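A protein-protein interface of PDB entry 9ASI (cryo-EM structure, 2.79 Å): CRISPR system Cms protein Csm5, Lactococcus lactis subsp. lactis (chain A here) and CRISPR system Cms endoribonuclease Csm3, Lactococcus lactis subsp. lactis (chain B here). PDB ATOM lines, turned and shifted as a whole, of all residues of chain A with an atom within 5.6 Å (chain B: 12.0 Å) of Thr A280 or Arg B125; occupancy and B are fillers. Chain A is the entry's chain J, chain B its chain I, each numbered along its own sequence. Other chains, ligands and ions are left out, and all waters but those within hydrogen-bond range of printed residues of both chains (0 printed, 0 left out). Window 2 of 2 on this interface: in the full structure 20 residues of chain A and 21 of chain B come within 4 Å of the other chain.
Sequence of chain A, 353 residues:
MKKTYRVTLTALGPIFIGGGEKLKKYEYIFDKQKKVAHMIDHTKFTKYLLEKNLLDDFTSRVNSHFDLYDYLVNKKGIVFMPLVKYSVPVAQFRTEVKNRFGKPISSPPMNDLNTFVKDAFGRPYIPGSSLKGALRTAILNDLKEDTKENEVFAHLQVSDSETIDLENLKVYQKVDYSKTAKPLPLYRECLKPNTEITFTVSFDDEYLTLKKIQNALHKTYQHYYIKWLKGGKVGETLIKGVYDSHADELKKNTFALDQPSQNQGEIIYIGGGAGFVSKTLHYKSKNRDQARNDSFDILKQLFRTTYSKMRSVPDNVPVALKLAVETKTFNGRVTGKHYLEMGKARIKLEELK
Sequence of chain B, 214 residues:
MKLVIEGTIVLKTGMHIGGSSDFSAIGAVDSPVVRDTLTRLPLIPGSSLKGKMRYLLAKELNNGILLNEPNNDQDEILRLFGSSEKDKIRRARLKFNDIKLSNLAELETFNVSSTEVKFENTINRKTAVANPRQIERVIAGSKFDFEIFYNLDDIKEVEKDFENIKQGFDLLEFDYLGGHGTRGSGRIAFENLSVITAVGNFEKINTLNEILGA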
ATOM      1  N   THR A 137      -6.945 -15.454 -17.475  1.00  0.00           N
ATOM      2  CA  THR A 137      -6.736 -16.821 -17.012  1.00  0.00           C
ATOM      3  C   THR A 137      -5.954 -17.654 -18.020  1.00  0.00           C
ATOM      4  O   THR A 137      -5.399 -18.693 -17.646  1.00  0.00           O
ATOM      5  CB  THR A 137      -8.068 -17.505 -16.682  1.00  0.00           C
ATOM      6  OG1 THR A 137      -7.823 -18.646 -15.850  1.00  0.00           O
ATOM      7  CG2 THR A 137      -8.772 -17.966 -17.940  1.00  0.00           C
ATOM      8  N   LYS A 144       1.547 -14.063 -11.048  1.00  0.00           N
ATOM      9  CA  LYS A 144       0.297 -13.804 -10.343  1.00  0.00           C
ATOM     10  C   LYS A 144       0.367 -12.481  -9.593  1.00  0.00           C
ATOM     11  O   LYS A 144      -0.062 -12.374  -8.440  1.00  0.00           O
ATOM     12  CB  LYS A 144      -0.037 -14.944  -9.384  1.00  0.00           C
ATOM     13  CG  LYS A 144       0.207 -16.335  -9.949  1.00  0.00           C
ATOM     14  CD  LYS A 144       0.728 -17.283  -8.878  1.00  0.00           C
ATOM     15  CE  LYS A 144       1.199 -18.595  -9.483  1.00  0.00           C
ATOM     16  NZ  LYS A 144       1.371 -19.646  -8.446  1.00  0.00           N
ATOM     17  N   PHE A 276     -14.961 -24.919 -12.651  1.00  0.00           N
ATOM     18  CA  PHE A 276     -14.224 -24.026 -11.765  1.00  0.00           C
ATOM     19  C   PHE A 276     -12.727 -24.030 -12.046  1.00  0.00           C
ATOM     20  O   PHE A 276     -11.998 -23.205 -11.482  1.00  0.00           O
ATOM     21  CB  PHE A 276     -14.518 -24.422 -10.309  1.00  0.00           C
ATOM     22  CG  PHE A 276     -13.855 -23.556  -9.271  1.00  0.00           C
ATOM     23  CD1 PHE A 276     -14.331 -22.285  -8.993  1.00  0.00           C
ATOM     24  CD2 PHE A 276     -12.815 -24.050  -8.505  1.00  0.00           C
ATOM     25  CE1 PHE A 276     -13.751 -21.503  -8.019  1.00  0.00           C
ATOM     26  CE2 PHE A 276     -12.231 -23.271  -7.526  1.00  0.00           C
ATOM     27  CZ  PHE A 276     -12.706 -21.997  -7.282  1.00  0.00           C
ATOM     28  N   VAL A 277     -12.256 -24.927 -12.917  1.00  0.00           N
ATOM     29  CA  VAL A 277     -10.843 -24.949 -13.277  1.00  0.00           C
ATOM     30  C   VAL A 277     -10.482 -23.730 -14.114  1.00  0.00           C
ATOM     31  O   VAL A 277      -9.403 -23.151 -13.956  1.00  0.00           O
ATOM     32  CB  VAL A 277     -10.499 -26.261 -14.005  1.00  0.00           C
ATOM     33  CG1 VAL A 277     -10.458 -27.408 -13.020  1.00  0.00           C
ATOM     34  CG2 VAL A 277     -11.512 -26.544 -15.101  1.00  0.00           C
ATOM     35  N   SER A 278     -11.375 -23.318 -15.016  1.00  0.00           N
ATOM     36  CA  SER A 278     -11.102 -22.154 -15.848  1.00  0.00           C
ATOM     37  C   SER A 278     -11.177 -20.849 -15.071  1.00  0.00           C
ATOM     38  O   SER A 278     -10.712 -19.821 -15.575  1.00  0.00           O
ATOM     39  CB  SER A 278     -12.075 -22.112 -17.029  1.00  0.00           C
ATOM     40  OG  SER A 278     -11.992 -23.301 -17.794  1.00  0.00           O
ATOM     41  N   LYS A 279     -11.748 -20.860 -13.867  1.00  0.00           N
ATOM     42  CA  LYS A 279     -11.861 -19.654 -13.059  1.00  0.00           C
ATOM     43  C   LYS A 279     -10.616 -19.414 -12.212  1.00  0.00           C
ATOM     44  O   LYS A 279     -10.146 -18.276 -12.112  1.00  0.00           O
ATOM     45  CB  LYS A 279     -13.093 -19.744 -12.155  1.00  0.00           C
ATOM     46  CG  LYS A 279     -13.283 -18.551 -11.241  1.00  0.00           C
ATOM     47  CD  LYS A 279     -13.809 -17.360 -12.009  1.00  0.00           C
ATOM     48  CE  LYS A 279     -14.416 -16.345 -11.071  1.00  0.00           C
ATOM     49  NZ  LYS A 279     -13.399 -15.766 -10.159  1.00  0.00           N
ATOM     50  N   THR A 280     -10.069 -20.470 -11.612  1.00  0.00           N
ATOM     51  CA  THR A 280      -8.904 -20.376 -10.739  1.00  0.00           C
ATOM     52  C   THR A 280      -7.662 -20.849 -11.487  1.00  0.00           C
ATOM     53  O   THR A 280      -7.637 -21.965 -12.015  1.00  0.00           O
ATOM     54  CB  THR A 280      -9.108 -21.196  -9.467  1.00  0.00           C
ATOM     55  OG1 THR A 280      -9.687 -22.467  -9.796  1.00  0.00           O
ATOM     56  CG2 THR A 280     -10.006 -20.451  -8.497  1.00  0.00           C
ATOM     57  N   LEU A 281      -6.633 -20.004 -11.517  1.00  0.00           N
ATOM     58  CA  LEU A 281      -5.418 -20.256 -12.291  1.00  0.00           C
ATOM     59  C   LEU A 281      -4.222 -20.398 -11.342  1.00  0.00           C
ATOM     60  O   LEU A 281      -3.519 -19.434 -11.029  1.00  0.00           O
ATOM     61  CB  LEU A 281      -5.225 -19.140 -13.362  1.00  0.00           C
ATOM     62  CG  LEU A 281      -4.801 -17.698 -13.049  1.00  0.00           C
ATOM     63  CD1 LEU A 281      -4.348 -16.980 -14.312  1.00  0.00           C
ATOM     64  CD2 LEU A 281      -5.921 -16.930 -12.371  1.00  0.00           C
ATOM     65  N   HIS A 282      -4.012 -21.624 -10.859  1.00  0.00           N
ATOM     66  CA  HIS A 282      -2.782 -21.985 -10.164  1.00  0.00           C
ATOM     67  C   HIS A 282      -2.231 -23.336 -10.592  1.00  0.00           C
ATOM     68  O   HIS A 282      -1.070 -23.627 -10.291  1.00  0.00           O
ATOM     69  CB  HIS A 282      -2.989 -21.989  -8.641  1.00  0.00           C
ATOM     70  CG  HIS A 282      -3.934 -23.046  -8.156  1.00  0.00           C
ATOM     71  ND1 HIS A 282      -5.252 -22.787  -7.850  1.00  0.00           N
ATOM     72  CD2 HIS A 282      -3.748 -24.367  -7.919  1.00  0.00           C
ATOM     73  CE1 HIS A 282      -5.838 -23.901  -7.446  1.00  0.00           C
ATOM     74  NE2 HIS A 282      -4.947 -24.874  -7.480  1.00  0.00           N
ATOM     75  N   TYR A 283      -3.010 -24.161 -11.290  1.00  0.00           N
ATOM     76  CA  TYR A 283      -2.619 -25.513 -11.666  1.00  0.00           C
ATOM     77  C   TYR A 283      -1.909 -25.575 -13.010  1.00  0.00           C
ATOM     78  O   TYR A 283      -1.628 -26.675 -13.498  1.00  0.00           O
ATOM     79  CB  TYR A 283      -3.850 -26.429 -11.682  1.00  0.00           C
ATOM     80  CG  TYR A 283      -4.914 -26.030 -12.679  1.00  0.00           C
ATOM     81  CD1 TYR A 283      -5.797 -24.995 -12.406  1.00  0.00           C
ATOM     82  CD2 TYR A 283      -5.045 -26.699 -13.887  1.00  0.00           C
ATOM     83  CE1 TYR A 283      -6.768 -24.631 -13.312  1.00  0.00           C
ATOM     84  CE2 TYR A 283      -6.016 -26.342 -14.798  1.00  0.00           C
ATOM     85  CZ  TYR A 283      -6.875 -25.307 -14.505  1.00  0.00           C
ATOM     86  OH  TYR A 283      -7.844 -24.948 -15.409  1.00  0.00           O
ATOM     87  N   ILE A 298      -7.464 -23.415  -0.936  1.00  0.00           N
ATOM     88  CA  ILE A 298      -8.242 -22.235  -1.307  1.00  0.00           C
ATOM     89  C   ILE A 298      -9.743 -22.519  -1.344  1.00  0.00           C
ATOM     90  O   ILE A 298     -10.540 -21.588  -1.183  1.00  0.00           O
ATOM     91  CB  ILE A 298      -7.752 -21.667  -2.652  1.00  0.00           C
ATOM     92  CG1 ILE A 298      -8.306 -20.259  -2.887  1.00  0.00           C
ATOM     93  CG2 ILE A 298      -8.156 -22.567  -3.805  1.00  0.00           C
ATOM     94  CD1 ILE A 298      -7.618 -19.514  -4.011  1.00  0.00           C
ATOM     95  N   MET A 310     -13.295 -30.883  -9.576  1.00  0.00           N
ATOM     96  CA  MET A 310     -14.515 -30.206 -10.001  1.00  0.00           C
ATOM     97  C   MET A 310     -15.161 -31.006 -11.126  1.00  0.00           C
ATOM     98  O   MET A 310     -14.667 -31.009 -12.259  1.00  0.00           O
ATOM     99  CB  MET A 310     -14.197 -28.781 -10.445  1.00  0.00           C
ATOM    100  CG  MET A 310     -13.938 -27.821  -9.296  1.00  0.00           C
ATOM    101  SD  MET A 310     -12.414 -28.182  -8.402  1.00  0.00           S
ATOM    102  CE  MET A 310     -11.199 -27.394  -9.453  1.00  0.00           C
ATOM    103  N   ASN B 121     -19.408  -7.699 -14.440  1.00  0.00           N
ATOM    104  CA  ASN B 121     -19.017  -8.338 -13.179  1.00  0.00           C
ATOM    105  C   ASN B 121     -17.908  -7.531 -12.503  1.00  0.00           C
ATOM    106  O   ASN B 121     -17.430  -6.543 -13.069  1.00  0.00           O
ATOM    107  CB  ASN B 121     -18.564  -9.780 -13.409  1.00  0.00           C
ATOM    108  CG  ASN B 121     -18.628 -10.610 -12.168  1.00  0.00           C
ATOM    109  OD1 ASN B 121     -18.866 -10.098 -11.081  1.00  0.00           O
ATOM    110  ND2 ASN B 121     -18.507 -11.919 -12.335  1.00  0.00           N
ATOM    111  N   THR B 122     -17.501  -7.919 -11.293  1.00  0.00           N
ATOM    112  CA  THR B 122     -16.189  -7.553 -10.739  1.00  0.00           C
ATOM    113  C   THR B 122     -15.604  -8.738  -9.962  1.00  0.00           C
ATOM    114  O   THR B 122     -15.158  -8.608  -8.821  1.00  0.00           O
ATOM    115  CB  THR B 122     -16.265  -6.305  -9.865  1.00  0.00           C
ATOM    116  OG1 THR B 122     -17.082  -5.322 -10.512  1.00  0.00           O
ATOM    117  CG2 THR B 122     -14.873  -5.710  -9.669  1.00  0.00           C
ATOM    118  N   ILE B 123     -15.630  -9.925 -10.567  1.00  0.00           N
ATOM    119  CA  ILE B 123     -15.403 -11.160  -9.822  1.00  0.00           C
ATOM    120  C   ILE B 123     -13.915 -11.349  -9.533  1.00  0.00           C
ATOM    121  O   ILE B 123     -13.048 -10.692 -10.115  1.00  0.00           O
ATOM    122  CB  ILE B 123     -15.983 -12.355 -10.592  1.00  0.00           C
ATOM    123  CG1 ILE B 123     -16.395 -13.475  -9.637  1.00  0.00           C
ATOM    124  CG2 ILE B 123     -14.984 -12.854 -11.623  1.00  0.00           C
ATOM    125  CD1 ILE B 123     -17.374 -14.445 -10.253  1.00  0.00           C
ATOM    126  N   ASN B 124     -13.620 -12.267  -8.606  1.00  0.00           N
ATOM    127  CA  ASN B 124     -12.264 -12.526  -8.138  1.00  0.00           C
ATOM    128  C   ASN B 124     -12.016 -14.024  -8.007  1.00  0.00           C
ATOM    129  O   ASN B 124     -12.891 -14.770  -7.560  1.00  0.00           O
ATOM    130  CB  ASN B 124     -12.003 -11.852  -6.782  1.00  0.00           C
ATOM    131  CG  ASN B 124     -12.086 -10.342  -6.854  1.00  0.00           C
ATOM    132  OD1 ASN B 124     -13.152  -9.778  -7.098  1.00  0.00           O
ATOM    133  ND2 ASN B 124     -10.959  -9.679  -6.640  1.00  0.00           N
ATOM    134  N   ARG B 125     -10.809 -14.456  -8.396  1.00  0.00           N
ATOM    135  CA  ARG B 125     -10.399 -15.843  -8.179  1.00  0.00           C
ATOM    136  C   ARG B 125     -10.186 -16.130  -6.699  1.00  0.00           C
ATOM    137  O   ARG B 125     -10.377 -17.267  -6.249  1.00  0.00           O
ATOM    138  CB  ARG B 125      -9.125 -16.146  -8.973  1.00  0.00           C
ATOM    139  CG  ARG B 125      -8.271 -17.273  -8.406  1.00  0.00           C
ATOM    140  CD  ARG B 125      -6.805 -17.127  -8.777  1.00  0.00           C
ATOM    141  NE  ARG B 125      -6.218 -15.913  -8.222  1.00  0.00           N
ATOM    142  CZ  ARG B 125      -5.086 -15.366  -8.644  1.00  0.00           C
ATOM    143  NH1 ARG B 125      -4.372 -15.914  -9.613  1.00  0.00           N
ATOM    144  NH2 ARG B 125      -4.658 -14.242  -8.078  1.00  0.00           N
ATOM    145  N   LYS B 126      -9.847 -15.101  -5.924  1.00  0.00           N
ATOM    146  CA  LYS B 126      -9.639 -15.202  -4.484  1.00  0.00           C
ATOM    147  C   LYS B 126     -10.996 -15.296  -3.803  1.00  0.00           C
ATOM    148  O   LYS B 126     -11.974 -15.679  -4.453  1.00  0.00           O
ATOM    149  CB  LYS B 126      -8.842 -14.006  -3.961  1.00  0.00           C
ATOM    150  CG  LYS B 126      -7.345 -14.098  -4.218  1.00  0.00           C
ATOM    151  CD  LYS B 126      -6.792 -15.461  -3.823  1.00  0.00           C
ATOM    152  CE  LYS B 126      -6.780 -15.643  -2.311  1.00  0.00           C
ATOM    153  NZ  LYS B 126      -6.991 -17.061  -1.908  1.00  0.00           N
ATOM    154  N   THR B 127     -11.055 -15.022  -2.499  1.00  0.00           N
ATOM    155  CA  THR B 127     -12.300 -15.116  -1.747  1.00  0.00           C
ATOM    156  C   THR B 127     -13.450 -14.541  -2.557  1.00  0.00           C
ATOM    157  O   THR B 127     -13.457 -13.354  -2.894  1.00  0.00           O
ATOM    158  CB  THR B 127     -12.170 -14.361  -0.421  1.00  0.00           C
ATOM    159  OG1 THR B 127     -11.699 -13.031  -0.671  1.00  0.00           O
ATOM    160  CG2 THR B 127     -11.197 -15.067   0.509  1.00  0.00           C
ATOM    161  N   ALA B 128     -14.424 -15.392  -2.873  1.00  0.00           N
ATOM    162  CA  ALA B 128     -15.320 -15.140  -3.994  1.00  0.00           C
ATOM    163  C   ALA B 128     -16.290 -14.004  -3.705  1.00  0.00           C
ATOM    164  O   ALA B 128     -17.373 -14.226  -3.155  1.00  0.00           O
ATOM    165  CB  ALA B 128     -16.089 -16.414  -4.351  1.00  0.00           C
ATOM    166  N   VAL B 129     -15.910 -12.788  -4.084  1.00  0.00           N
ATOM    167  CA  VAL B 129     -16.760 -11.615  -3.936  1.00  0.00           C
ATOM    168  C   VAL B 129     -16.742 -10.842  -5.245  1.00  0.00           C
ATOM    169  O   VAL B 129     -15.672 -10.581  -5.806  1.00  0.00           O
ATOM    170  CB  VAL B 129     -16.315 -10.719  -2.763  1.00  0.00           C
ATOM    171  CG1 VAL B 129     -16.708 -11.355  -1.437  1.00  0.00           C
ATOM    172  CG2 VAL B 129     -14.815 -10.461  -2.816  1.00  0.00           C
ATOM    173  N   ALA B 130     -17.925 -10.489  -5.734  1.00  0.00           N
ATOM    174  CA  ALA B 130     -18.084  -9.726  -6.960  1.00  0.00           C
ATOM    175  C   ALA B 130     -18.751  -8.400  -6.635  1.00  0.00           C
ATOM    176  O   ALA B 130     -19.622  -8.331  -5.765  1.00  0.00           O
ATOM    177  CB  ALA B 130     -18.912 -10.497  -7.987  1.00  0.00           C
ATOM    178  N   ASN B 131     -18.337  -7.343  -7.335  1.00  0.00           N
ATOM    179  CA  ASN B 131     -18.864  -5.997  -7.123  1.00  0.00           C
ATOM    180  C   ASN B 131     -19.546  -5.547  -8.408  1.00  0.00           C
ATOM    181  O   ASN B 131     -18.915  -4.926  -9.277  1.00  0.00           O
ATOM    182  CB  ASN B 131     -17.754  -5.033  -6.714  1.00  0.00           C
ATOM    183  CG  ASN B 131     -18.287  -3.705  -6.221  1.00  0.00           C
ATOM    184  OD1 ASN B 131     -19.429  -3.606  -5.773  1.00  0.00           O
ATOM    185  ND2 ASN B 131     -17.459  -2.673  -6.299  1.00  0.00           N
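The backbone NH (N) of Ile B123 lies within hydrogen-bond range of the side-chain amide oxygen (OD1) of Asn B121, at 3.3 Å.
O of Val B129 lies close to OD1 of Asn B124.
O of Thr B122 lies close to OD1 of Asn B124.
The backbone carbonyl oxygen (O) of Phe A276 sits at hydrogen-bond distance from the side-chain hydroxyl (OG1) of Thr A280 (3.0 Å).
Thr A280 touches just one residue of chain B: Arg B125.
Arg B125 touches just these residues of chain A: Lys A279, Thr A280 and Leu A281.
No residue of chain B comes within 4 Å of Phe A276.
No residue of chain B comes within 4 Å of Ser A278.
No residue of chain B comes within 4 Å of His A282.
No residue of chain B comes within 4 Å of Tyr A283.
Of the printed residues of chain B, Ile A298 touches Lys B126.
Printed residues of chain A within 4 Å of Asn B124: Lys A279 (2.8 Å).
The side-chain amino group (NZ) of Lys A279 lies close to the backbone NH (N) of Arg B125, 3.4 Å away.
The backbone carbonyl oxygen of Asn B124 is in hydrogen-bond range of the side-chain amino group of Lys A279 (2.8 Å).
Printed residues of chain B that touch a printed residue of chain A: Ile B123, Asn B124, Arg B125 and Lys B126.
Hydrophobic or aromatic side chains of chain A within 4 Å of the printed part of chain B: Leu A281 and Ile A298.
Among the printed residues, 6 pairs touch across the chains.
Among the printed residues, no Asp or Glu carboxylate lies within 4 Å of a Lys or Arg side-chain nitrogen of the other chain.
Among the printed residues, pairs that only touch across the chains: Lys A279 with Ile B123 (3.6 Å), Thr A280 with Arg B125 (3.6 Å), Leu A281 with Arg B125 (3.3 Å) and Ile A298 with Lys B126 (3.3 Å).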
